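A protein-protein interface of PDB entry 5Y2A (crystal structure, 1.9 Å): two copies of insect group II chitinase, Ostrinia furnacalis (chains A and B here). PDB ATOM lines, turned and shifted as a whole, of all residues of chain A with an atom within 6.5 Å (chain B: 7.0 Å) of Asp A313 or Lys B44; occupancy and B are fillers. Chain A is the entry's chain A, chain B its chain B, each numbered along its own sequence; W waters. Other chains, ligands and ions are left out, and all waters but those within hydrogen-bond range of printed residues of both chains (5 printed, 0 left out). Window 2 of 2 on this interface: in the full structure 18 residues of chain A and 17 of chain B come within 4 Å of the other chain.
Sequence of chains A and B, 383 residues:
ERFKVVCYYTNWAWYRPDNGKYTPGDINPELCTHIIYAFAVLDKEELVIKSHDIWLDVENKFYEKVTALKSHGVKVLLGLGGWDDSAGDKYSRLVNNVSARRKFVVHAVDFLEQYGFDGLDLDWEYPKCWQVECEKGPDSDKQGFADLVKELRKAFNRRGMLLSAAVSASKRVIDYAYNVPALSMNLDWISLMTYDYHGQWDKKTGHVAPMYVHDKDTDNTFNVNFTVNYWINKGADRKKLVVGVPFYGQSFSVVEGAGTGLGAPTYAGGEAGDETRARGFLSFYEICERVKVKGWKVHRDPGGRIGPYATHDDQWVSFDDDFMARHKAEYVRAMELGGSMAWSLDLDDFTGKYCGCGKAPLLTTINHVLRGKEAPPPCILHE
Water W3 lies within hydrogen-bond range of the side-chain carboxylate (OD1) of Asp B89 (2.5 Å), the side-chain hydroxyl (OH) of Tyr A267 (2.9 Å), the side-chain carboxylate (OD2) of Asp A314 (2.9 Å) and the side-chain amino group (NZ) of Lys B44 (3.1 Å). Water W4 lies within hydrogen-bond range of O of Ala B87 (2.5 Å) and OE2 of Glu A271 (3.4 Å). Water W5 lies within hydrogen-bond range of the side-chain carboxylate of Glu A271 (2.6 Å), the backbone NH of Lys B44 (2.8 Å) and the side-chain amino group of Lys B50 (3.3 Å). Water W2 lies within hydrogen-bond range of the side-chain carboxylate of Glu A271 (2.6 Å) and the side-chain amino group of Lys B44 (2.6 Å). Water W1 bridges NE of Arg B93 (2.7 Å) and OD1 of Asp A313 (2.9 Å).
Among the printed residues, merely in contact across the chains: Tyr A267 with Gly B88 (3.3 Å), Tyr A267 with Ala B87 (3.7 Å), Gln A315 with Lys B44 (3.8 Å) and Glu A271 with Lys B44 (3.9 Å).
Asp A313 touches just one residue of chain B: Lys B44. Lys B44 touches just these residues of chain A: Glu A271 (3.9 Å), Asp A313 (3.3 Å), Asp A314 (2.8 Å) and Gln A315 (3.8 Å). Of the printed residues of chain A, Lys B90 touches Glu A271. Of the printed residues of chain B, Gln A315 touches Lys B44 (3.8 Å). Leu B47 touches none of the printed residues of chain A. The nearest residue of chain B that does not touch Asp A313 is Asp B89 (5.3 Å). The nearest residue of chain A that does not touch Lys B44 is Tyr A267 (4.5 Å).
Hydrophobic or aromatic side chains of chain B that line the printed part of chain A: Ala B87. Of the 12 printed residues of chain A, 6 touch a printed residue of chain B. Printed residues of chain A that touch a printed residue of chain B: Tyr A267, Glu A271, His A312, Asp A313, Asp A314 and Gln A315. Among the printed residues, Asp or Glu carboxylates within 4 Å of a Lys or Arg side-chain nitrogen of the other chain: Glu A271 with Lys B90, Asp A313 with Lys B44 and Asp A314 with Lys B44.
N of Val A254 lies within hydrogen-bond range of O of Asp A314. N of Glu A271 sits at hydrogen-bond distance from OE1 of Gln A315, at 2.8 Å. The backbone carbonyl oxygen (O) of Lys B44 sits at hydrogen-bond distance from the guanidinium group (NH2) of Arg B93 (2.8 Å). NZ of Lys B90 lies within hydrogen-bond range of O of Leu B42 (2.7 Å). The side-chain carboxylate (OD2) of Asp A314 sits at hydrogen-bond distance from the side-chain hydroxyl (OH) of Tyr A267 (2.6 Å). The side-chain carboxylate (OD2) of Asp B43 sits close to the backbone NH (N) of Glu B45, at 3.4 Å.
No position is printed for both chains. Of the 8 pairs that touch across the chains among the printed residues, none has its exchanged pair printed and touching as well.
The side-chain carboxylate (OD1) of Asp A314 is in salt-bridge range of the side-chain amino group (NZ) of Lys B44, 2.8 Å away. The side-chain carboxylate (OD2) of Asp A313 is in salt-bridge range of the side-chain amino group (NZ) of Lys B44 (3.6 Å). The side-chain amino group (NZ) of Lys B90 lies within salt-bridge range of the side-chain carboxylate (OE1) of Glu A271, 3.1 Å away. The side-chain carboxylate of Glu B45 sits at hydrogen-bond distance from a ring nitrogen (NE2) of His A312.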
ATOM      1  N   SER A 253     -21.977  -7.212  27.954  1.00  0.00           N
ATOM      2  CA  SER A 253     -20.618  -7.239  27.417  1.00  0.00           C
ATOM      3  C   SER A 253     -20.389  -5.931  26.661  1.00  0.00           C
ATOM      4  O   SER A 253     -21.140  -5.618  25.733  1.00  0.00           O
ATOM      5  CB  SER A 253     -20.412  -8.452  26.510  1.00  0.00           C
ATOM      6  OG  SER A 253     -20.593  -9.668  27.235  1.00  0.00           O
ATOM      7  N   VAL A 254     -19.354  -5.167  27.063  1.00  0.00           N
ATOM      8  CA  VAL A 254     -19.159  -3.792  26.599  1.00  0.00           C
ATOM      9  C   VAL A 254     -18.231  -3.769  25.388  1.00  0.00           C
ATOM     10  O   VAL A 254     -17.219  -4.481  25.345  1.00  0.00           O
ATOM     11  CB  VAL A 254     -18.605  -2.909  27.736  1.00  0.00           C
ATOM     12  CG1 VAL A 254     -18.439  -1.445  27.262  1.00  0.00           C
ATOM     13  CG2 VAL A 254     -19.527  -2.959  28.964  1.00  0.00           C
ATOM     14  N   GLY A 259     -15.070   1.972  27.700  1.00  0.00           N
ATOM     15  CA  GLY A 259     -15.027   2.332  29.102  1.00  0.00           C
ATOM     16  C   GLY A 259     -16.007   1.535  29.944  1.00  0.00           C
ATOM     17  O   GLY A 259     -16.641   0.579  29.495  1.00  0.00           O
ATOM     18  N   THR A 260     -16.138   1.960  31.202  1.00  0.00           N
ATOM     19  CA  THR A 260     -16.974   1.258  32.172  1.00  0.00           C
ATOM     20  C   THR A 260     -18.145   2.094  32.665  1.00  0.00           C
ATOM     21  O   THR A 260     -18.787   1.715  33.650  1.00  0.00           O
ATOM     22  CB  THR A 260     -16.137   0.804  33.373  1.00  0.00           C
ATOM     23  OG1 THR A 260     -15.581   1.952  34.034  1.00  0.00           O
ATOM     24  CG2 THR A 260     -15.023  -0.118  32.926  1.00  0.00           C
ATOM     25  N   TYR A 267     -22.449  -5.032  23.126  1.00  0.00           N
ATOM     26  CA  TYR A 267     -22.665  -5.912  21.991  1.00  0.00           C
ATOM     27  C   TYR A 267     -23.370  -7.218  22.339  1.00  0.00           C
ATOM     28  O   TYR A 267     -23.744  -7.958  21.421  1.00  0.00           O
ATOM     29  CB  TYR A 267     -21.325  -6.228  21.305  1.00  0.00           C
ATOM     30  CG  TYR A 267     -20.359  -7.019  22.163  1.00  0.00           C
ATOM     31  CD1 TYR A 267     -20.386  -8.407  22.175  1.00  0.00           C
ATOM     32  CD2 TYR A 267     -19.416  -6.377  22.956  1.00  0.00           C
ATOM     33  CE1 TYR A 267     -19.516  -9.133  22.954  1.00  0.00           C
ATOM     34  CE2 TYR A 267     -18.526  -7.102  23.739  1.00  0.00           C
ATOM     35  CZ  TYR A 267     -18.582  -8.480  23.731  1.00  0.00           C
ATOM     36  OH  TYR A 267     -17.707  -9.214  24.512  1.00  0.00           O
ATOM     37  N   GLU A 271     -21.549 -12.725  30.081  1.00  0.00           N
ATOM     38  CA  GLU A 271     -21.332 -14.158  30.272  1.00  0.00           C
ATOM     39  C   GLU A 271     -22.286 -14.708  31.325  1.00  0.00           C
ATOM     40  O   GLU A 271     -22.554 -14.059  32.341  1.00  0.00           O
ATOM     41  CB  GLU A 271     -19.886 -14.420  30.719  1.00  0.00           C
ATOM     42  CG  GLU A 271     -18.795 -14.147  29.692  1.00  0.00           C
ATOM     43  CD  GLU A 271     -18.787 -15.174  28.567  1.00  0.00           C
ATOM     44  OE1 GLU A 271     -18.941 -16.375  28.868  1.00  0.00           O
ATOM     45  OE2 GLU A 271     -18.627 -14.788  27.396  1.00  0.00           O
ATOM     46  N   THR A 311     -17.780  -4.406  37.502  1.00  0.00           N
ATOM     47  CA  THR A 311     -17.120  -4.544  36.216  1.00  0.00           C
ATOM     48  C   THR A 311     -15.874  -5.419  36.324  1.00  0.00           C
ATOM     49  O   THR A 311     -15.231  -5.496  37.370  1.00  0.00           O
ATOM     50  CB  THR A 311     -16.699  -3.191  35.627  1.00  0.00           C
ATOM     51  OG1 THR A 311     -15.772  -2.563  36.521  1.00  0.00           O
ATOM     52  CG2 THR A 311     -17.915  -2.288  35.390  1.00  0.00           C
ATOM     53  N   HIS A 312     -15.554  -6.068  35.202  1.00  0.00           N
ATOM     54  CA  HIS A 312     -14.348  -6.853  35.012  1.00  0.00           C
ATOM     55  C   HIS A 312     -14.189  -7.087  33.522  1.00  0.00           C
ATOM     56  O   HIS A 312     -15.115  -7.577  32.873  1.00  0.00           O
ATOM     57  CB  HIS A 312     -14.424  -8.194  35.756  1.00  0.00           C
ATOM     58  CG  HIS A 312     -13.193  -9.030  35.630  1.00  0.00           C
ATOM     59  ND1 HIS A 312     -12.062  -8.827  36.394  1.00  0.00           N
ATOM     60  CD2 HIS A 312     -12.914 -10.076  34.813  1.00  0.00           C
ATOM     61  CE1 HIS A 312     -11.142  -9.716  36.062  1.00  0.00           C
ATOM     62  NE2 HIS A 312     -11.632 -10.484  35.103  1.00  0.00           N
ATOM     63  N   ASP A 313     -13.004  -6.758  32.988  1.00  0.00           N
ATOM     64  CA  ASP A 313     -12.738  -6.797  31.542  1.00  0.00           C
ATOM     65  C   ASP A 313     -13.885  -6.045  30.861  1.00  0.00           C
ATOM     66  O   ASP A 313     -14.203  -4.925  31.288  1.00  0.00           O
ATOM     67  CB  ASP A 313     -12.536  -8.229  31.092  1.00  0.00           C
ATOM     68  CG  ASP A 313     -12.069  -8.322  29.658  1.00  0.00           C
ATOM     69  OD1 ASP A 313     -10.876  -8.073  29.388  1.00  0.00           O
ATOM     70  OD2 ASP A 313     -12.919  -8.578  28.781  1.00  0.00           O
ATOM     71  N   ASP A 314     -14.557  -6.625  29.855  1.00  0.00           N
ATOM     72  CA  ASP A 314     -15.678  -5.980  29.211  1.00  0.00           C
ATOM     73  C   ASP A 314     -17.030  -6.389  29.809  1.00  0.00           C
ATOM     74  O   ASP A 314     -18.077  -6.119  29.202  1.00  0.00           O
ATOM     75  CB  ASP A 314     -15.659  -6.233  27.685  1.00  0.00           C
ATOM     76  CG  ASP A 314     -15.928  -7.686  27.309  1.00  0.00           C
ATOM     77  OD1 ASP A 314     -16.065  -8.564  28.185  1.00  0.00           O
ATOM     78  OD2 ASP A 314     -16.000  -7.963  26.094  1.00  0.00           O
ATOM     79  N   GLN A 315     -17.016  -6.988  30.997  1.00  0.00           N
ATOM     80  CA  GLN A 315     -18.256  -7.409  31.657  1.00  0.00           C
ATOM     81  C   GLN A 315     -18.742  -6.305  32.590  1.00  0.00           C
ATOM     82  O   GLN A 315     -17.939  -5.595  33.204  1.00  0.00           O
ATOM     83  CB  GLN A 315     -18.041  -8.697  32.446  1.00  0.00           C
ATOM     84  CG  GLN A 315     -17.635  -9.901  31.600  1.00  0.00           C
ATOM     85  CD  GLN A 315     -18.674 -10.227  30.547  1.00  0.00           C
ATOM     86  OE1 GLN A 315     -19.745 -10.754  30.857  1.00  0.00           O
ATOM     87  NE2 GLN A 315     -18.377  -9.891  29.297  1.00  0.00           N
ATOM     88  N   TRP A 316     -20.059  -6.197  32.720  1.00  0.00           N
ATOM     89  CA  TRP A 316     -20.698  -5.053  33.369  1.00  0.00           C
ATOM     90  C   TRP A 316     -22.072  -5.497  33.849  1.00  0.00           C
ATOM     91  O   TRP A 316     -22.881  -5.952  33.039  1.00  0.00           O
ATOM     92  CB  TRP A 316     -20.813  -3.910  32.362  1.00  0.00           C
ATOM     93  CG  TRP A 316     -21.076  -2.523  32.881  1.00  0.00           C
ATOM     94  CD1 TRP A 316     -20.174  -1.502  32.963  1.00  0.00           C
ATOM     95  CD2 TRP A 316     -22.338  -1.979  33.301  1.00  0.00           C
ATOM     96  NE1 TRP A 316     -20.789  -0.364  33.436  1.00  0.00           N
ATOM     97  CE2 TRP A 316     -22.116  -0.630  33.651  1.00  0.00           C
ATOM     98  CE3 TRP A 316     -23.634  -2.507  33.428  1.00  0.00           C
ATOM     99  CZ2 TRP A 316     -23.135   0.200  34.132  1.00  0.00           C
ATOM    100  CZ3 TRP A 316     -24.646  -1.683  33.894  1.00  0.00           C
ATOM    101  CH2 TRP A 316     -24.392  -0.340  34.246  1.00  0.00           C
ATOM    102  N   VAL B  41     -19.137 -24.255  26.317  1.00  0.00           N
ATOM    103  CA  VAL B  41     -18.754 -22.868  26.072  1.00  0.00           C
ATOM    104  C   VAL B  41     -17.292 -22.683  26.442  1.00  0.00           C
ATOM    105  O   VAL B  41     -16.695 -23.483  27.168  1.00  0.00           O
ATOM    106  CB  VAL B  41     -19.602 -21.837  26.852  1.00  0.00           C
ATOM    107  CG1 VAL B  41     -21.048 -21.882  26.419  1.00  0.00           C
ATOM    108  CG2 VAL B  41     -19.480 -22.044  28.338  1.00  0.00           C
ATOM    109  N   LEU B  42     -16.722 -21.587  25.949  1.00  0.00           N
ATOM    110  CA  LEU B  42     -15.338 -21.244  26.246  1.00  0.00           C
ATOM    111  C   LEU B  42     -15.337 -20.319  27.453  1.00  0.00           C
ATOM    112  O   LEU B  42     -15.941 -19.243  27.410  1.00  0.00           O
ATOM    113  CB  LEU B  42     -14.667 -20.572  25.046  1.00  0.00           C
ATOM    114  CG  LEU B  42     -13.166 -20.277  25.174  1.00  0.00           C
ATOM    115  CD1 LEU B  42     -12.332 -21.550  25.200  1.00  0.00           C
ATOM    116  CD2 LEU B  42     -12.706 -19.351  24.055  1.00  0.00           C
ATOM    117  N   ASP B  43     -14.686 -20.742  28.537  1.00  0.00           N
ATOM    118  CA  ASP B  43     -14.587 -19.871  29.702  1.00  0.00           C
ATOM    119  C   ASP B  43     -13.835 -18.600  29.341  1.00  0.00           C
ATOM    120  O   ASP B  43     -12.745 -18.652  28.768  1.00  0.00           O
ATOM    121  CB  ASP B  43     -13.897 -20.574  30.865  1.00  0.00           C
ATOM    122  CG  ASP B  43     -13.908 -19.721  32.124  1.00  0.00           C
ATOM    123  OD1 ASP B  43     -15.015 -19.466  32.631  1.00  0.00           O
ATOM    124  OD2 ASP B  43     -12.827 -19.314  32.599  1.00  0.00           O
ATOM    125  N   LYS B  44     -14.447 -17.454  29.646  1.00  0.00           N
ATOM    126  CA  LYS B  44     -13.872 -16.181  29.225  1.00  0.00           C
ATOM    127  C   LYS B  44     -12.532 -15.924  29.900  1.00  0.00           C
ATOM    128  O   LYS B  44     -11.581 -15.461  29.256  1.00  0.00           O
ATOM    129  CB  LYS B  44     -14.853 -15.045  29.520  1.00  0.00           C
ATOM    130  CG  LYS B  44     -14.333 -13.676  29.120  1.00  0.00           C
ATOM    131  CD  LYS B  44     -15.195 -12.563  29.685  1.00  0.00           C
ATOM    132  CE  LYS B  44     -14.811 -11.225  29.081  1.00  0.00           C
ATOM    133  NZ  LYS B  44     -15.115 -11.163  27.627  1.00  0.00           N
ATOM    134  N   GLU B  45     -12.411 -16.293  31.174  1.00  0.00           N
ATOM    135  CA  GLU B  45     -11.220 -15.959  31.942  1.00  0.00           C
ATOM    136  C   GLU B  45     -10.094 -16.957  31.678  1.00  0.00           C
ATOM    137  O   GLU B  45      -8.957 -16.554  31.412  1.00  0.00           O
ATOM    138  CB  GLU B  45     -11.569 -15.895  33.431  1.00  0.00           C
ATOM    139  CG  GLU B  45     -10.439 -15.450  34.359  1.00  0.00           C
ATOM    140  CD  GLU B  45     -10.015 -13.993  34.172  1.00  0.00           C
ATOM    141  OE1 GLU B  45     -10.794 -13.180  33.622  1.00  0.00           O
ATOM    142  OE2 GLU B  45      -8.886 -13.657  34.592  1.00  0.00           O
ATOM    143  N   GLU B  46     -10.385 -18.260  31.752  1.00  0.00           N
ATOM    144  CA  GLU B  46      -9.366 -19.291  31.568  1.00  0.00           C
ATOM    145  C   GLU B  46      -9.155 -19.707  30.117  1.00  0.00           C
ATOM    146  O   GLU B  46      -8.130 -20.332  29.815  1.00  0.00           O
ATOM    147  CB  GLU B  46      -9.706 -20.543  32.389  1.00  0.00           C
ATOM    148  CG  GLU B  46      -9.775 -20.324  33.889  1.00  0.00           C
ATOM    149  CD  GLU B  46      -8.440 -19.904  34.475  1.00  0.00           C
ATOM    150  OE1 GLU B  46      -7.396 -20.196  33.855  1.00  0.00           O
ATOM    151  OE2 GLU B  46      -8.434 -19.287  35.560  1.00  0.00           O
ATOM    152  N   LEU B  47     -10.093 -19.394  29.220  1.00  0.00           N
ATOM    153  CA  LEU B  47     -10.012 -19.802  27.813  1.00  0.00           C
ATOM    154  C   LEU B  47      -9.841 -21.316  27.677  1.00  0.00           C
ATOM    155  O   LEU B  47      -8.967 -21.816  26.960  1.00  0.00           O
ATOM    156  CB  LEU B  47      -8.898 -19.049  27.080  1.00  0.00           C
ATOM    157  CG  LEU B  47      -9.034 -17.525  27.090  1.00  0.00           C
ATOM    158  CD1 LEU B  47      -7.866 -16.849  26.355  1.00  0.00           C
ATOM    159  CD2 LEU B  47     -10.371 -17.093  26.483  1.00  0.00           C
ATOM    160  N   VAL B  48     -10.707 -22.057  28.378  1.00  0.00           N
ATOM    161  CA  VAL B  48     -10.782 -23.507  28.266  1.00  0.00           C
ATOM    162  C   VAL B  48     -12.249 -23.905  28.164  1.00  0.00           C
ATOM    163  O   VAL B  48     -13.150 -23.133  28.501  1.00  0.00           O
ATOM    164  CB  VAL B  48     -10.113 -24.233  29.456  1.00  0.00           C
ATOM    165  CG1 VAL B  48      -8.624 -23.873  29.554  1.00  0.00           C
ATOM    166  CG2 VAL B  48     -10.855 -23.927  30.762  1.00  0.00           C
ATOM    167  N   LYS B  50     -15.734 -25.346  29.078  1.00  0.00           N
ATOM    168  CA  LYS B  50     -16.479 -25.576  30.306  1.00  0.00           C
ATOM    169  C   LYS B  50     -17.934 -25.893  29.987  1.00  0.00           C
ATOM    170  O   LYS B  50     -18.439 -25.557  28.912  1.00  0.00           O
ATOM    171  CB  LYS B  50     -16.392 -24.377  31.259  1.00  0.00           C
ATOM    172  CG  LYS B  50     -17.271 -23.219  30.883  1.00  0.00           C
ATOM    173  CD  LYS B  50     -17.353 -22.207  32.012  1.00  0.00           C
ATOM    174  CE  LYS B  50     -18.037 -20.931  31.533  1.00  0.00           C
ATOM    175  NZ  LYS B  50     -17.914 -19.829  32.532  1.00  0.00           N
ATOM    176  N   ALA B  87     -20.212 -14.238  20.507  1.00  0.00           N
ATOM    177  CA  ALA B  87     -20.118 -12.788  20.598  1.00  0.00           C
ATOM    178  C   ALA B  87     -18.831 -12.391  21.315  1.00  0.00           C
ATOM    179  O   ALA B  87     -18.423 -13.023  22.293  1.00  0.00           O
ATOM    180  CB  ALA B  87     -21.334 -12.211  21.325  1.00  0.00           C
ATOM    181  N   GLY B  88     -18.187 -11.345  20.825  1.00  0.00           N
ATOM    182  CA  GLY B  88     -17.001 -10.856  21.501  1.00  0.00           C
ATOM    183  C   GLY B  88     -15.742 -11.586  21.090  1.00  0.00           C
ATOM    184  O   GLY B  88     -15.731 -12.434  20.195  1.00  0.00           O
ATOM    185  N   ASP B  89     -14.663 -11.279  21.809  1.00  0.00           N
ATOM    186  CA  ASP B  89     -13.314 -11.584  21.352  1.00  0.00           C
ATOM    187  C   ASP B  89     -12.683 -12.811  22.006  1.00  0.00           C
ATOM    188  O   ASP B  89     -11.499 -13.067  21.772  1.00  0.00           O
ATOM    189  CB  ASP B  89     -12.409 -10.364  21.566  1.00  0.00           C
ATOM    190  CG  ASP B  89     -12.148 -10.053  23.042  1.00  0.00           C
ATOM    191  OD1 ASP B  89     -12.670 -10.747  23.936  1.00  0.00           O
ATOM    192  OD2 ASP B  89     -11.390  -9.098  23.306  1.00  0.00           O
ATOM    193  N   LYS B  90     -13.418 -13.567  22.827  1.00  0.00           N
ATOM    194  CA  LYS B  90     -12.746 -14.588  23.630  1.00  0.00           C
ATOM    195  C   LYS B  90     -12.135 -15.691  22.766  1.00  0.00           C
ATOM    196  O   LYS B  90     -11.022 -16.151  23.049  1.00  0.00           O
ATOM    197  CB  LYS B  90     -13.685 -15.170  24.693  1.00  0.00           C
ATOM    198  CG  LYS B  90     -14.940 -15.882  24.206  1.00  0.00           C
ATOM    199  CD  LYS B  90     -15.705 -16.410  25.437  1.00  0.00           C
ATOM    200  CE  LYS B  90     -17.029 -17.058  25.053  1.00  0.00           C
ATOM    201  NZ  LYS B  90     -17.789 -17.589  26.237  1.00  0.00           N
ATOM    202  N   ARG B  93      -9.004 -14.171  21.302  1.00  0.00           N
ATOM    203  CA  ARG B  93      -7.895 -14.120  22.245  1.00  0.00           C
ATOM    204  C   ARG B  93      -7.248 -15.483  22.397  1.00  0.00           C
ATOM    205  O   ARG B  93      -6.022 -15.576  22.539  1.00  0.00           O
ATOM    206  CB  ARG B  93      -8.360 -13.613  23.611  1.00  0.00           C
ATOM    207  CG  ARG B  93      -8.787 -12.156  23.603  1.00  0.00           C
ATOM    208  CD  ARG B  93      -8.949 -11.608  25.005  1.00  0.00           C
ATOM    209  NE  ARG B  93     -10.083 -12.192  25.706  1.00  0.00           N
ATOM    210  CZ  ARG B  93      -9.985 -13.106  26.669  1.00  0.00           C
ATOM    211  NH1 ARG B  93      -8.798 -13.548  27.061  1.00  0.00           N
ATOM    212  NH2 ARG B  93     -11.083 -13.570  27.250  1.00  0.00           N
HETATM  213  O   HOH W   1     -10.349 -10.352  27.605  1.00  0.00           O
HETATM  214  O   HOH W   2     -17.051 -12.769  26.820  1.00  0.00           O
HETATM  215  O   HOH W   3     -15.019 -10.285  24.632  1.00  0.00           O
HETATM  216  O   HOH W   4     -19.624 -14.264  24.161  1.00  0.00           O
HETATM  217  O   HOH W   5     -17.208 -17.525  30.346  1.00  0.00           O
